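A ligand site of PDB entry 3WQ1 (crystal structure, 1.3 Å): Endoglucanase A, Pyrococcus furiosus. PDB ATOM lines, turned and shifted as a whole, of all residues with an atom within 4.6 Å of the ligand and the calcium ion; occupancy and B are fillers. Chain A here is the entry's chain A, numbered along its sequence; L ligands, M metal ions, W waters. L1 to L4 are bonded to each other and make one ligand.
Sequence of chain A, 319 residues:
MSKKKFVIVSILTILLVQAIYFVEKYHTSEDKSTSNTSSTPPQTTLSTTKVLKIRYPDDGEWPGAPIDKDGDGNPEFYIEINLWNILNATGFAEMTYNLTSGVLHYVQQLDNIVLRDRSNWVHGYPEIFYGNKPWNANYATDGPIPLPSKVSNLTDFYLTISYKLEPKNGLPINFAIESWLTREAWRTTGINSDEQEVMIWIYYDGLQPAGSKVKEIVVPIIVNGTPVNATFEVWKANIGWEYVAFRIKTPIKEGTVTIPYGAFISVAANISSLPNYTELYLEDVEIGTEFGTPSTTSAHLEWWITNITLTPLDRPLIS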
ATOM      1  N   TRP A  62      18.384 -17.932  18.610  1.00  0.00           N
ATOM      2  CA  TRP A  62      17.296 -17.021  18.738  1.00  0.00           C
ATOM      3  C   TRP A  62      16.100 -17.736  19.386  1.00  0.00           C
ATOM      4  O   TRP A  62      15.006 -17.837  18.792  1.00  0.00           O
ATOM      5  CB  TRP A  62      16.832 -16.522  17.356  1.00  0.00           C
ATOM      6  CG  TRP A  62      17.921 -15.694  16.609  1.00  0.00           C
ATOM      7  CD1 TRP A  62      18.524 -16.057  15.476  1.00  0.00           C
ATOM      8  CD2 TRP A  62      18.433 -14.434  16.987  1.00  0.00           C
ATOM      9  NE1 TRP A  62      19.398 -15.101  15.100  1.00  0.00           N
ATOM     10  CE2 TRP A  62      19.322 -14.040  15.966  1.00  0.00           C
ATOM     11  CE3 TRP A  62      18.127 -13.525  17.972  1.00  0.00           C
ATOM     12  CZ2 TRP A  62      19.999 -12.821  15.982  1.00  0.00           C
ATOM     13  CZ3 TRP A  62      18.789 -12.265  17.994  1.00  0.00           C
ATOM     14  CH2 TRP A  62      19.723 -11.964  17.025  1.00  0.00           C
ATOM     15  N   GLU A  80      10.826 -13.759  23.592  1.00  0.00           N
ATOM     16  CA  GLU A  80      12.124 -13.966  22.927  1.00  0.00           C
ATOM     17  C   GLU A  80      13.229 -13.733  23.962  1.00  0.00           C
ATOM     18  O   GLU A  80      13.166 -12.733  24.660  1.00  0.00           O
ATOM     19  CB  GLU A  80      12.363 -13.026  21.759  1.00  0.00           C
ATOM     20  CG  GLU A  80      11.391 -13.148  20.602  1.00  0.00           C
ATOM     21  CD  GLU A  80      11.685 -12.213  19.434  1.00  0.00           C
ATOM     22  OE1 GLU A  80      12.687 -11.483  19.528  1.00  0.00           O
ATOM     23  OE2 GLU A  80      10.865 -12.212  18.492  1.00  0.00           O
ATOM     24  N   ASN A  82      16.337 -13.100  22.823  1.00  0.00           N
ATOM     25  CA  ASN A  82      16.819 -11.923  22.079  1.00  0.00           C
ATOM     26  C   ASN A  82      18.176 -11.416  22.568  1.00  0.00           C
ATOM     27  O   ASN A  82      18.347 -10.207  22.825  1.00  0.00           O
ATOM     28  CB  ASN A  82      15.753 -10.807  22.038  1.00  0.00           C
ATOM     29  CG  ASN A  82      16.128  -9.722  21.074  1.00  0.00           C
ATOM     30  OD1 ASN A  82      16.809  -9.976  20.045  1.00  0.00           O
ATOM     31  ND2 ASN A  82      15.598  -8.507  21.281  1.00  0.00           N
ATOM     32  N   TRP A  84      20.725 -10.275  21.119  1.00  0.00           N
ATOM     33  CA  TRP A  84      21.034  -9.918  19.727  1.00  0.00           C
ATOM     34  C   TRP A  84      22.419  -9.398  19.560  1.00  0.00           C
ATOM     35  O   TRP A  84      22.905  -9.424  18.426  1.00  0.00           O
ATOM     36  CB  TRP A  84      19.963  -8.977  19.176  1.00  0.00           C
ATOM     37  CG  TRP A  84      19.880  -7.653  19.914  1.00  0.00           C
ATOM     38  CD1 TRP A  84      19.056  -7.311  20.945  1.00  0.00           C
ATOM     39  CD2 TRP A  84      20.661  -6.458  19.644  1.00  0.00           C
ATOM     40  NE1 TRP A  84      19.251  -6.013  21.380  1.00  0.00           N
ATOM     41  CE2 TRP A  84      20.230  -5.473  20.560  1.00  0.00           C
ATOM     42  CE3 TRP A  84      21.613  -6.140  18.674  1.00  0.00           C
ATOM     43  CZ2 TRP A  84      20.716  -4.131  20.521  1.00  0.00           C
ATOM     44  CZ3 TRP A  84      22.081  -4.815  18.636  1.00  0.00           C
ATOM     45  CH2 TRP A  84      21.618  -3.839  19.535  1.00  0.00           C
ATOM     46  N   VAL A 122      24.547  -2.341  24.466  1.00  0.00           N
ATOM     47  CA  VAL A 122      23.898  -3.399  25.270  1.00  0.00           C
ATOM     48  C   VAL A 122      24.148  -4.728  24.642  1.00  0.00           C
ATOM     49  O   VAL A 122      24.569  -4.888  23.517  1.00  0.00           O
ATOM     50  CB  VAL A 122      22.386  -3.130  25.413  1.00  0.00           C
ATOM     51  CG1 VAL A 122      22.189  -1.811  26.191  1.00  0.00           C
ATOM     52  CG2 VAL A 122      21.657  -3.108  24.043  1.00  0.00           C
ATOM     53  N   GLY A 124      21.647  -7.395  24.784  1.00  0.00           N
ATOM     54  CA  GLY A 124      20.458  -8.090  24.366  1.00  0.00           C
ATOM     55  C   GLY A 124      19.260  -7.430  25.029  1.00  0.00           C
ATOM     56  O   GLY A 124      19.372  -6.511  25.821  1.00  0.00           O
ATOM     57  N   TYR A 125      18.090  -7.981  24.731  1.00  0.00           N
ATOM     58  CA  TYR A 125      16.788  -7.436  25.178  1.00  0.00           C
ATOM     59  C   TYR A 125      15.804  -8.616  25.283  1.00  0.00           C
ATOM     60  O   TYR A 125      14.860  -8.735  24.506  1.00  0.00           O
ATOM     61  CB  TYR A 125      16.326  -6.378  24.175  1.00  0.00           C
ATOM     62  CG  TYR A 125      15.001  -5.676  24.442  1.00  0.00           C
ATOM     63  CD1 TYR A 125      14.738  -4.992  25.619  1.00  0.00           C
ATOM     64  CD2 TYR A 125      14.017  -5.664  23.465  1.00  0.00           C
ATOM     65  CE1 TYR A 125      13.551  -4.283  25.812  1.00  0.00           C
ATOM     66  CE2 TYR A 125      12.839  -4.982  23.652  1.00  0.00           C
ATOM     67  CZ  TYR A 125      12.598  -4.282  24.803  1.00  0.00           C
ATOM     68  OH  TYR A 125      11.405  -3.612  24.921  1.00  0.00           O
ATOM     69  N   GLU A 127      12.571 -10.352  26.317  1.00  0.00           N
ATOM     70  CA  GLU A 127      11.345  -9.576  26.183  1.00  0.00           C
ATOM     71  C   GLU A 127      10.107 -10.440  25.946  1.00  0.00           C
ATOM     72  O   GLU A 127      10.194 -11.617  25.570  1.00  0.00           O
ATOM     73  CB  GLU A 127      11.493  -8.588  24.984  1.00  0.00           C
ATOM     74  CG  GLU A 127      11.693  -9.354  23.643  1.00  0.00           C
ATOM     75  CD  GLU A 127      11.698  -8.392  22.524  1.00  0.00           C
ATOM     76  OE1 GLU A 127      10.652  -7.679  22.364  1.00  0.00           O
ATOM     77  OE2 GLU A 127      12.651  -8.320  21.747  1.00  0.00           O
ATOM     78  N   ASN A 132       3.256  -7.123  15.871  1.00  0.00           N
ATOM     79  CA  ASN A 132       4.194  -7.697  14.902  1.00  0.00           C
ATOM     80  C   ASN A 132       5.572  -7.135  15.130  1.00  0.00           C
ATOM     81  O   ASN A 132       5.806  -5.931  14.901  1.00  0.00           O
ATOM     82  CB  ASN A 132       3.742  -7.377  13.475  1.00  0.00           C
ATOM     83  CG  ASN A 132       4.818  -7.732  12.508  1.00  0.00           C
ATOM     84  OD1 ASN A 132       5.380  -8.832  12.581  1.00  0.00           O
ATOM     85  ND2 ASN A 132       5.150  -6.816  11.566  1.00  0.00           N
ATOM     86  N   LYS A 133       6.504  -7.936  15.623  1.00  0.00           N
ATOM     87  CA  LYS A 133       7.883  -7.410  15.793  1.00  0.00           C
ATOM     88  C   LYS A 133       8.482  -7.335  14.414  1.00  0.00           C
ATOM     89  O   LYS A 133       8.538  -8.319  13.669  1.00  0.00           O
ATOM     90  CB  LYS A 133       8.707  -8.336  16.694  1.00  0.00           C
ATOM     91  CG  LYS A 133      10.154  -7.843  16.834  1.00  0.00           C
ATOM     92  CD  LYS A 133      10.901  -8.519  17.988  1.00  0.00           C
ATOM     93  CE  LYS A 133      12.350  -8.122  17.975  1.00  0.00           C
ATOM     94  NZ  LYS A 133      13.147  -8.780  19.046  1.00  0.00           N
ATOM     95  N   PRO A 134       9.061  -6.151  13.975  1.00  0.00           N
ATOM     96  CA  PRO A 134       9.338  -5.984  12.561  1.00  0.00           C
ATOM     97  C   PRO A 134      10.724  -6.483  12.177  1.00  0.00           C
ATOM     98  O   PRO A 134      11.084  -6.449  10.991  1.00  0.00           O
ATOM     99  CB  PRO A 134       9.288  -4.462  12.330  1.00  0.00           C
ATOM    100  CG  PRO A 134       9.725  -3.921  13.742  1.00  0.00           C
ATOM    101  CD  PRO A 134       8.975  -4.859  14.713  1.00  0.00           C
ATOM    102  N   TRP A 135      11.494  -7.054  13.112  1.00  0.00           N
ATOM    103  CA  TRP A 135      12.794  -7.625  12.876  1.00  0.00           C
ATOM    104  C   TRP A 135      12.780  -9.096  12.502  1.00  0.00           C
ATOM    105  O   TRP A 135      13.823  -9.643  12.166  1.00  0.00           O
ATOM    106  CB  TRP A 135      13.697  -7.411  14.126  1.00  0.00           C
ATOM    107  CG  TRP A 135      14.040  -5.988  14.317  1.00  0.00           C
ATOM    108  CD1 TRP A 135      13.445  -5.066  15.152  1.00  0.00           C
ATOM    109  CD2 TRP A 135      15.087  -5.257  13.604  1.00  0.00           C
ATOM    110  NE1 TRP A 135      14.040  -3.789  15.006  1.00  0.00           N
ATOM    111  CE2 TRP A 135      15.045  -3.915  14.084  1.00  0.00           C
ATOM    112  CE3 TRP A 135      16.015  -5.647  12.609  1.00  0.00           C
ATOM    113  CZ2 TRP A 135      15.963  -2.938  13.604  1.00  0.00           C
ATOM    114  CZ3 TRP A 135      16.939  -4.628  12.126  1.00  0.00           C
ATOM    115  CH2 TRP A 135      16.834  -3.308  12.617  1.00  0.00           C
ATOM    116  N   ASN A 136      11.601  -9.741  12.594  1.00  0.00           N
ATOM    117  CA  ASN A 136      11.540 -11.194  12.370  1.00  0.00           C
ATOM    118  C   ASN A 136      10.104 -11.539  12.026  1.00  0.00           C
ATOM    119  O   ASN A 136       9.220 -10.680  11.901  1.00  0.00           O
ATOM    120  CB  ASN A 136      12.125 -11.963  13.564  1.00  0.00           C
ATOM    121  CG  ASN A 136      11.396 -11.683  14.842  1.00  0.00           C
ATOM    122  OD1 ASN A 136      10.148 -11.539  14.841  1.00  0.00           O
ATOM    123  ND2 ASN A 136      12.131 -11.655  15.982  1.00  0.00           N
ATOM    124  N   ALA A 137       9.840 -12.858  11.874  1.00  0.00           N
ATOM    125  CA  ALA A 137       8.520 -13.330  11.494  1.00  0.00           C
ATOM    126  C   ALA A 137       7.691 -13.703  12.719  1.00  0.00           C
ATOM    127  O   ALA A 137       6.702 -14.439  12.565  1.00  0.00           O
ATOM    128  CB  ALA A 137       8.662 -14.525  10.514  1.00  0.00           C
ATOM    129  N   ASN A 138       7.998 -13.165  13.896  1.00  0.00           N
ATOM    130  CA  ASN A 138       7.225 -13.451  15.073  1.00  0.00           C
ATOM    131  C   ASN A 138       6.162 -12.432  15.317  1.00  0.00           C
ATOM    132  O   ASN A 138       6.379 -11.181  15.081  1.00  0.00           O
ATOM    133  CB  ASN A 138       8.154 -13.542  16.309  1.00  0.00           C
ATOM    134  CG  ASN A 138       9.190 -14.615  16.160  1.00  0.00           C
ATOM    135  OD1 ASN A 138       8.959 -15.613  15.418  1.00  0.00           O
ATOM    136  ND2 ASN A 138      10.300 -14.477  16.826  1.00  0.00           N
ATOM    137  N   TYR A 139       5.021 -12.813  15.835  1.00  0.00           N
ATOM    138  CA  TYR A 139       3.878 -11.916  16.024  1.00  0.00           C
ATOM    139  C   TYR A 139       2.923 -12.462  17.038  1.00  0.00           C
ATOM    140  O   TYR A 139       2.903 -13.683  17.326  1.00  0.00           O
ATOM    141  CB  TYR A 139       3.094 -11.684  14.663  1.00  0.00           C
ATOM    142  CG  TYR A 139       2.438 -12.953  14.158  1.00  0.00           C
ATOM    143  CD1 TYR A 139       3.128 -13.872  13.371  1.00  0.00           C
ATOM    144  CD2 TYR A 139       1.099 -13.293  14.524  1.00  0.00           C
ATOM    145  CE1 TYR A 139       2.557 -15.074  12.979  1.00  0.00           C
ATOM    146  CE2 TYR A 139       0.524 -14.496  14.157  1.00  0.00           C
ATOM    147  CZ  TYR A 139       1.265 -15.374  13.370  1.00  0.00           C
ATOM    148  OH  TYR A 139       0.675 -16.560  13.004  1.00  0.00           O
ATOM    149  N   GLU A 178       8.924  -0.760  24.137  1.00  0.00           N
ATOM    150  CA  GLU A 178       9.201  -0.050  22.928  1.00  0.00           C
ATOM    151  C   GLU A 178       8.246  -0.395  21.838  1.00  0.00           C
ATOM    152  O   GLU A 178       7.626  -1.479  21.783  1.00  0.00           O
ATOM    153  CB  GLU A 178      10.592  -0.155  22.498  1.00  0.00           C
ATOM    154  CG  GLU A 178      10.990  -1.422  21.935  1.00  0.00           C
ATOM    155  CD  GLU A 178      12.325  -1.359  21.165  1.00  0.00           C
ATOM    156  OE1 GLU A 178      12.766  -0.159  20.883  1.00  0.00           O
ATOM    157  OE2 GLU A 178      13.066  -2.258  20.845  1.00  0.00           O
ATOM    158  N   TRP A 180       8.016   0.035  17.317  1.00  0.00           N
ATOM    159  CA  TRP A 180       8.589   0.373  16.043  1.00  0.00           C
ATOM    160  C   TRP A 180       7.481   0.915  15.148  1.00  0.00           C
ATOM    161  O   TRP A 180       6.382   0.354  15.093  1.00  0.00           O
ATOM    162  CB  TRP A 180       9.221  -0.840  15.398  1.00  0.00           C
ATOM    163  CG  TRP A 180      10.328  -1.405  16.209  1.00  0.00           C
ATOM    164  CD1 TRP A 180      10.228  -2.399  17.209  1.00  0.00           C
ATOM    165  CD2 TRP A 180      11.714  -1.006  16.211  1.00  0.00           C
ATOM    166  NE1 TRP A 180      11.452  -2.668  17.706  1.00  0.00           N
ATOM    167  CE2 TRP A 180      12.410  -1.834  17.149  1.00  0.00           C
ATOM    168  CE3 TRP A 180      12.453  -0.086  15.408  1.00  0.00           C
ATOM    169  CZ2 TRP A 180      13.759  -1.746  17.378  1.00  0.00           C
ATOM    170  CZ3 TRP A 180      13.823   0.000  15.674  1.00  0.00           C
ATOM    171  CH2 TRP A 180      14.475  -0.812  16.593  1.00  0.00           C
ATOM    172  N   ARG A 187       5.748  -5.324   8.536  1.00  0.00           N
ATOM    173  CA  ARG A 187       7.185  -5.399   8.212  1.00  0.00           C
ATOM    174  C   ARG A 187       7.846  -6.583   8.940  1.00  0.00           C
ATOM    175  O   ARG A 187       7.564  -6.809  10.126  1.00  0.00           O
ATOM    176  CB  ARG A 187       7.854  -4.129   8.756  1.00  0.00           C
ATOM    177  CG  ARG A 187       9.363  -4.102   8.676  1.00  0.00           C
ATOM    178  CD  ARG A 187       9.980  -4.114   7.291  1.00  0.00           C
ATOM    179  NE  ARG A 187       9.500  -3.006   6.450  1.00  0.00           N
ATOM    180  CZ  ARG A 187       9.740  -1.709   6.698  1.00  0.00           C
ATOM    181  NH1 ARG A 187      10.622  -1.383   7.689  1.00  0.00           N
ATOM    182  NH2 ARG A 187       9.127  -0.768   5.984  1.00  0.00           N
ATOM    183  N   THR A 188       8.702  -7.349   8.263  1.00  0.00           N
ATOM    184  CA  THR A 188       9.383  -8.449   8.937  1.00  0.00           C
ATOM    185  C   THR A 188      10.877  -8.548   8.652  1.00  0.00           C
ATOM    186  O   THR A 188      11.532  -9.459   9.058  1.00  0.00           O
ATOM    187  CB  THR A 188       8.701  -9.780   8.618  1.00  0.00           C
ATOM    188  OG1 THR A 188       8.718  -9.963   7.202  1.00  0.00           O
ATOM    189  CG2 THR A 188       7.255  -9.817   9.101  1.00  0.00           C
ATOM    190  N   GLU A 197      11.852   4.402  16.108  1.00  0.00           N
ATOM    191  CA  GLU A 197      11.865   3.537  17.259  1.00  0.00           C
ATOM    192  C   GLU A 197      11.496   4.391  18.445  1.00  0.00           C
ATOM    193  O   GLU A 197      12.131   5.470  18.664  1.00  0.00           O
ATOM    194  CB  GLU A 197      13.269   2.941  17.469  1.00  0.00           C
ATOM    195  CG  GLU A 197      13.337   1.947  18.645  1.00  0.00           C
ATOM    196  CD  GLU A 197      14.691   1.428  18.955  1.00  0.00           C
ATOM    197  OE1 GLU A 197      15.714   1.864  18.348  1.00  0.00           O
ATOM    198  OE2 GLU A 197      14.810   0.559  19.871  1.00  0.00           O
ATOM    199  N   MET A 199      11.143   4.217  22.626  1.00  0.00           N
ATOM    200  CA  MET A 199      11.193   3.457  23.866  1.00  0.00           C
ATOM    201  C   MET A 199      10.740   4.291  25.026  1.00  0.00           C
ATOM    202  O   MET A 199      10.933   5.536  25.084  1.00  0.00           O
ATOM    203  CB  MET A 199      12.623   3.040  24.205  1.00  0.00           C
ATOM    204  CG  MET A 199      13.420   2.626  23.003  1.00  0.00           C
ATOM    205  SD  MET A 199      15.040   1.992  23.525  1.00  0.00           S
ATOM    206  CE  MET A 199      14.591   0.326  24.056  1.00  0.00           C
ATOM    207  N   ILE A 239      20.182   6.734  14.398  1.00  0.00           N
ATOM    208  CA  ILE A 239      20.992   5.517  14.555  1.00  0.00           C
ATOM    209  C   ILE A 239      20.732   4.542  13.358  1.00  0.00           C
ATOM    210  O   ILE A 239      20.878   3.314  13.499  1.00  0.00           O
ATOM    211  CB  ILE A 239      20.761   4.840  15.903  1.00  0.00           C
ATOM    212  CG1 ILE A 239      19.280   4.473  16.102  1.00  0.00           C
ATOM    213  CG2 ILE A 239      21.304   5.780  17.000  1.00  0.00           C
ATOM    214  CD1 ILE A 239      19.125   3.600  17.305  1.00  0.00           C
ATOM    215  N   TRP A 241      17.774   4.973  11.848  1.00  0.00           N
ATOM    216  CA  TRP A 241      16.378   5.316  11.898  1.00  0.00           C
ATOM    217  C   TRP A 241      16.297   6.401  13.007  1.00  0.00           C
ATOM    218  O   TRP A 241      17.294   6.620  13.710  1.00  0.00           O
ATOM    219  CB  TRP A 241      15.437   4.089  12.245  1.00  0.00           C
ATOM    220  CG  TRP A 241      15.898   3.321  13.436  1.00  0.00           C
ATOM    221  CD1 TRP A 241      15.551   3.571  14.750  1.00  0.00           C
ATOM    222  CD2 TRP A 241      16.749   2.155  13.471  1.00  0.00           C
ATOM    223  NE1 TRP A 241      16.147   2.639  15.581  1.00  0.00           N
ATOM    224  CE2 TRP A 241      16.870   1.747  14.828  1.00  0.00           C
ATOM    225  CE3 TRP A 241      17.370   1.392  12.467  1.00  0.00           C
ATOM    226  CZ2 TRP A 241      17.623   0.619  15.187  1.00  0.00           C
ATOM    227  CZ3 TRP A 241      18.133   0.293  12.824  1.00  0.00           C
ATOM    228  CH2 TRP A 241      18.218  -0.116  14.208  1.00  0.00           C
ATOM    229  N   TYR A 243      15.332   7.642  16.564  1.00  0.00           N
ATOM    230  CA  TYR A 243      15.130   7.014  17.864  1.00  0.00           C
ATOM    231  C   TYR A 243      14.684   8.090  18.827  1.00  0.00           C
ATOM    232  O   TYR A 243      15.315   9.166  18.926  1.00  0.00           O
ATOM    233  CB  TYR A 243      16.496   6.455  18.303  1.00  0.00           C
ATOM    234  CG  TYR A 243      16.685   6.022  19.729  1.00  0.00           C
ATOM    235  CD1 TYR A 243      17.010   6.967  20.737  1.00  0.00           C
ATOM    236  CD2 TYR A 243      16.627   4.661  20.085  1.00  0.00           C
ATOM    237  CE1 TYR A 243      17.272   6.560  22.034  1.00  0.00           C
ATOM    238  CE2 TYR A 243      16.912   4.240  21.364  1.00  0.00           C
ATOM    239  CZ  TYR A 243      17.267   5.205  22.332  1.00  0.00           C
ATOM    240  OH  TYR A 243      17.603   4.825  23.612  1.00  0.00           O
HETATM  241  C1  LIG L   1      18.171  -0.301  19.835  1.00  0.00           C
HETATM  242  C2  LIG L   1      17.383  -1.316  19.033  1.00  0.00           C
HETATM  243  C3  LIG L   1      17.270  -2.639  19.852  1.00  0.00           C
HETATM  244  C4  LIG L   1      16.664  -2.325  21.191  1.00  0.00           C
HETATM  245  C5  LIG L   1      16.549  -3.483  22.109  1.00  0.00           C
HETATM  246  C6  LIG L   1      17.509   0.029  21.227  1.00  0.00           C
HETATM  247  O1  LIG L   1      18.443   0.686  21.968  1.00  0.00           O
HETATM  248  O2  LIG L   1      18.182   0.949  19.149  1.00  0.00           O
HETATM  249  O3  LIG L   1      18.005  -1.524  17.747  1.00  0.00           O
HETATM  250  O4  LIG L   1      16.405  -3.559  19.146  1.00  0.00           O
HETATM  251  O5  LIG L   1      17.514  -1.345  21.841  1.00  0.00           O
HETATM  252  O6  LIG L   1      17.863  -3.868  22.578  1.00  0.00           O
HETATM  253  C1  LG2 L   2      16.107  -5.730  18.148  1.00  0.00           C
HETATM  254  C2  LG2 L   2      16.917  -6.870  17.428  1.00  0.00           C
HETATM  255  C3  LG2 L   2      17.795  -6.285  16.291  1.00  0.00           C
HETATM  256  C4  LG2 L   2      18.548  -5.058  16.654  1.00  0.00           C
HETATM  257  C5  LG2 L   2      19.101  -4.322  15.432  1.00  0.00           C
HETATM  258  C6  LG2 L   2      17.093  -4.657  18.523  1.00  0.00           C
HETATM  259  O1  LG2 L   2      15.441  -6.288  19.312  1.00  0.00           O
HETATM  260  O2  LG2 L   2      15.950  -7.807  16.962  1.00  0.00           O
HETATM  261  O3  LG2 L   2      18.765  -7.204  15.867  1.00  0.00           O
HETATM  262  O4  LG2 L   2      17.680  -4.146  17.350  1.00  0.00           O
HETATM  263  O5  LG2 L   2      20.116  -3.376  15.819  1.00  0.00           O
HETATM  264  C1  LG3 L   3      15.494 -10.084  16.546  1.00  0.00           C
HETATM  265  C2  LG3 L   3      16.051 -11.345  15.868  1.00  0.00           C
HETATM  266  C3  LG3 L   3      16.406 -11.048  14.418  1.00  0.00           C
HETATM  267  C4  LG3 L   3      17.306  -9.857  14.391  1.00  0.00           C
HETATM  268  C5  LG3 L   3      17.733  -9.397  12.952  1.00  0.00           C
HETATM  269  C6  LG3 L   3      16.503  -9.012  16.416  1.00  0.00           C
HETATM  270  O1  LG3 L   3      15.191 -10.378  17.906  1.00  0.00           O
HETATM  271  O2  LG3 L   3      15.021 -12.345  15.942  1.00  0.00           O
HETATM  272  O3  LG3 L   3      17.134 -12.140  13.809  1.00  0.00           O
HETATM  273  O4  LG3 L   3      16.681  -8.744  15.016  1.00  0.00           O
HETATM  274  O5  LG3 L   3      18.713  -8.299  13.165  1.00  0.00           O
HETATM  275  C1  LG4 L   4      17.457 -13.771  12.145  1.00  0.00           C
HETATM  276  C2  LG4 L   4      16.728 -14.889  11.381  1.00  0.00           C
HETATM  277  C3  LG4 L   4      15.970 -15.832  12.334  1.00  0.00           C
HETATM  278  C4  LG4 L   4      15.017 -14.998  13.190  1.00  0.00           C
HETATM  279  C5  LG4 L   4      14.378 -15.826  14.261  1.00  0.00           C
HETATM  280  C6  LG4 L   4      16.373 -13.043  12.975  1.00  0.00           C
HETATM  281  O1  LG4 L   4      18.005 -12.828  11.204  1.00  0.00           O
HETATM  282  O2  LG4 L   4      17.732 -15.627  10.633  1.00  0.00           O
HETATM  283  O3  LG4 L   4      15.278 -16.821  11.585  1.00  0.00           O
HETATM  284  O4  LG4 L   4      15.804 -13.983  13.880  1.00  0.00           O
HETATM  285  O5  LG4 L   4      13.378 -15.017  14.886  1.00  0.00           O
HETATM  286 CA    CA M   1       7.286 -10.168  13.123  1.00  0.00          CA
HETATM  287  O   HOH W   1      14.499 -13.289  18.615  1.00  0.00           O
HETATM  288  O   HOH W   2      13.226  -4.806  19.613  1.00  0.00           O
HETATM  289  O   HOH W   3      15.029 -19.162  13.099  1.00  0.00           O
HETATM  290  O   HOH W   4      13.152 -15.518  17.622  1.00  0.00           O
HETATM  291  O   HOH W   5      18.800  -1.558  24.072  1.00  0.00           O
HETATM  292  O   HOH W   6      11.105 -15.308  13.255  1.00  0.00           O
HETATM  293  O   HOH W   7      20.079   2.474  20.511  1.00  0.00           O
HETATM  294  O   HOH W   8      19.479  -6.955  10.847  1.00  0.00           O
HETATM  295  O   HOH W   9       5.658 -11.485  11.912  1.00  0.00           O
HETATM  296  O   HOH W  10      20.486  -0.657  17.000  1.00  0.00           O
HETATM  297  O   HOH W  11      20.467 -11.924  12.063  1.00  0.00           O
HETATM  298  O   HOH W  12      21.663  -0.387  21.367  1.00  0.00           O
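The side-chain carboxylate of Glu 197 lies within hydrogen-bond range of an oxygen (O2) of LIG L1, at 2.8 Å.
An oxygen (O1) of LG3 L3 is in hydrogen-bond range of the side-chain amide oxygen (OD1) of Asn 82 (2.7 Å).
OE1 of Glu 80 sits at hydrogen-bond distance from O1 of LG3 L3 (3.2 Å).
The side-chain amino group (NZ) of Lys 133 lies within hydrogen-bond range of an oxygen (O1) of LG3 L3.
O2 of LG3 L3 is in hydrogen-bond range of ND2 of Asn 136 (3.0 Å).
NE1 of Trp 84 is in hydrogen-bond range of O6 of LIG L1.
The backbone NH of Tyr 125 sits at hydrogen-bond distance from the backbone carbonyl oxygen of Asn 82, 2.9 Å away.
OE2 of Glu 127 lies within salt-bridge range of NZ of Lys 133 (2.8 Å).
OD1 of Asn 136 lies within hydrogen-bond range of N of Asn 138, 2.9 Å away.
ND2 of Asn 82 sits close to NZ of Lys 133, at 3.3 Å.
OE1 of Glu 197 lies within hydrogen-bond range of NE1 of Trp 241, 2.9 Å away.
NZ of Lys 133 is in salt-bridge range of OE1 of Glu 80, at 2.8 Å.
The backbone NH (N) of Glu 127 is in hydrogen-bond range of the backbone carbonyl oxygen (O) of Glu 80 (3.0 Å).
OE2 of Glu 127 lies within hydrogen-bond range of ND2 of Asn 82 (3.0 Å).
Merely in contact with the ligand: Trp 62 (3.6 Å), Tyr 125 (3.3 Å), Trp 135 (3.4 Å), Glu 178 (3.6 Å), Trp 180 (3.7 Å), Met 199 (3.9 Å), Ile 239 (3.4 Å), Trp 241 (3.4 Å) and Tyr 243 (3.9 Å).
The nearest printed residue that does not touch the ligand is Val 122 (4.1 Å).
Ala 137 touches the calcium ion.
Of the 25 residues printed, 5 come within 4 Å of the calcium ion.
The calcium ion is bound by the backbone carbonyl oxygen of Lys 133 (2.3 Å), the backbone carbonyl oxygen of Asn 136 (2.3 Å), the backbone carbonyl oxygen of Asn 138 (2.4 Å), the side-chain amide oxygen of Asn 132 (2.4 Å) and water W9 (2.4 Å).
The calcium ion has five donor atoms within binding distance.
Water W2 lies within hydrogen-bond range of O1 of LG2 L2 (2.7 Å), OE2 of Glu 178 (2.8 Å) and NE1 of Trp 180 (3.4 Å).
Water W4 lies within hydrogen-bond range of an oxygen (O5) of LG4 L4, the side-chain amide nitrogen (ND2) of Asn 138 and the backbone carbonyl oxygen (O) of Trp 62.
Water W6 lies within hydrogen-bond range of O5 of LG4 L4 (2.8 Å), OD1 of Asn 138 (3.1 Å) and N of Ala 137 (3.1 Å).
Water W1 lies within hydrogen-bond range of OE1 of Glu 80 (2.7 Å) and O2 of LG3 L3 (2.9 Å).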
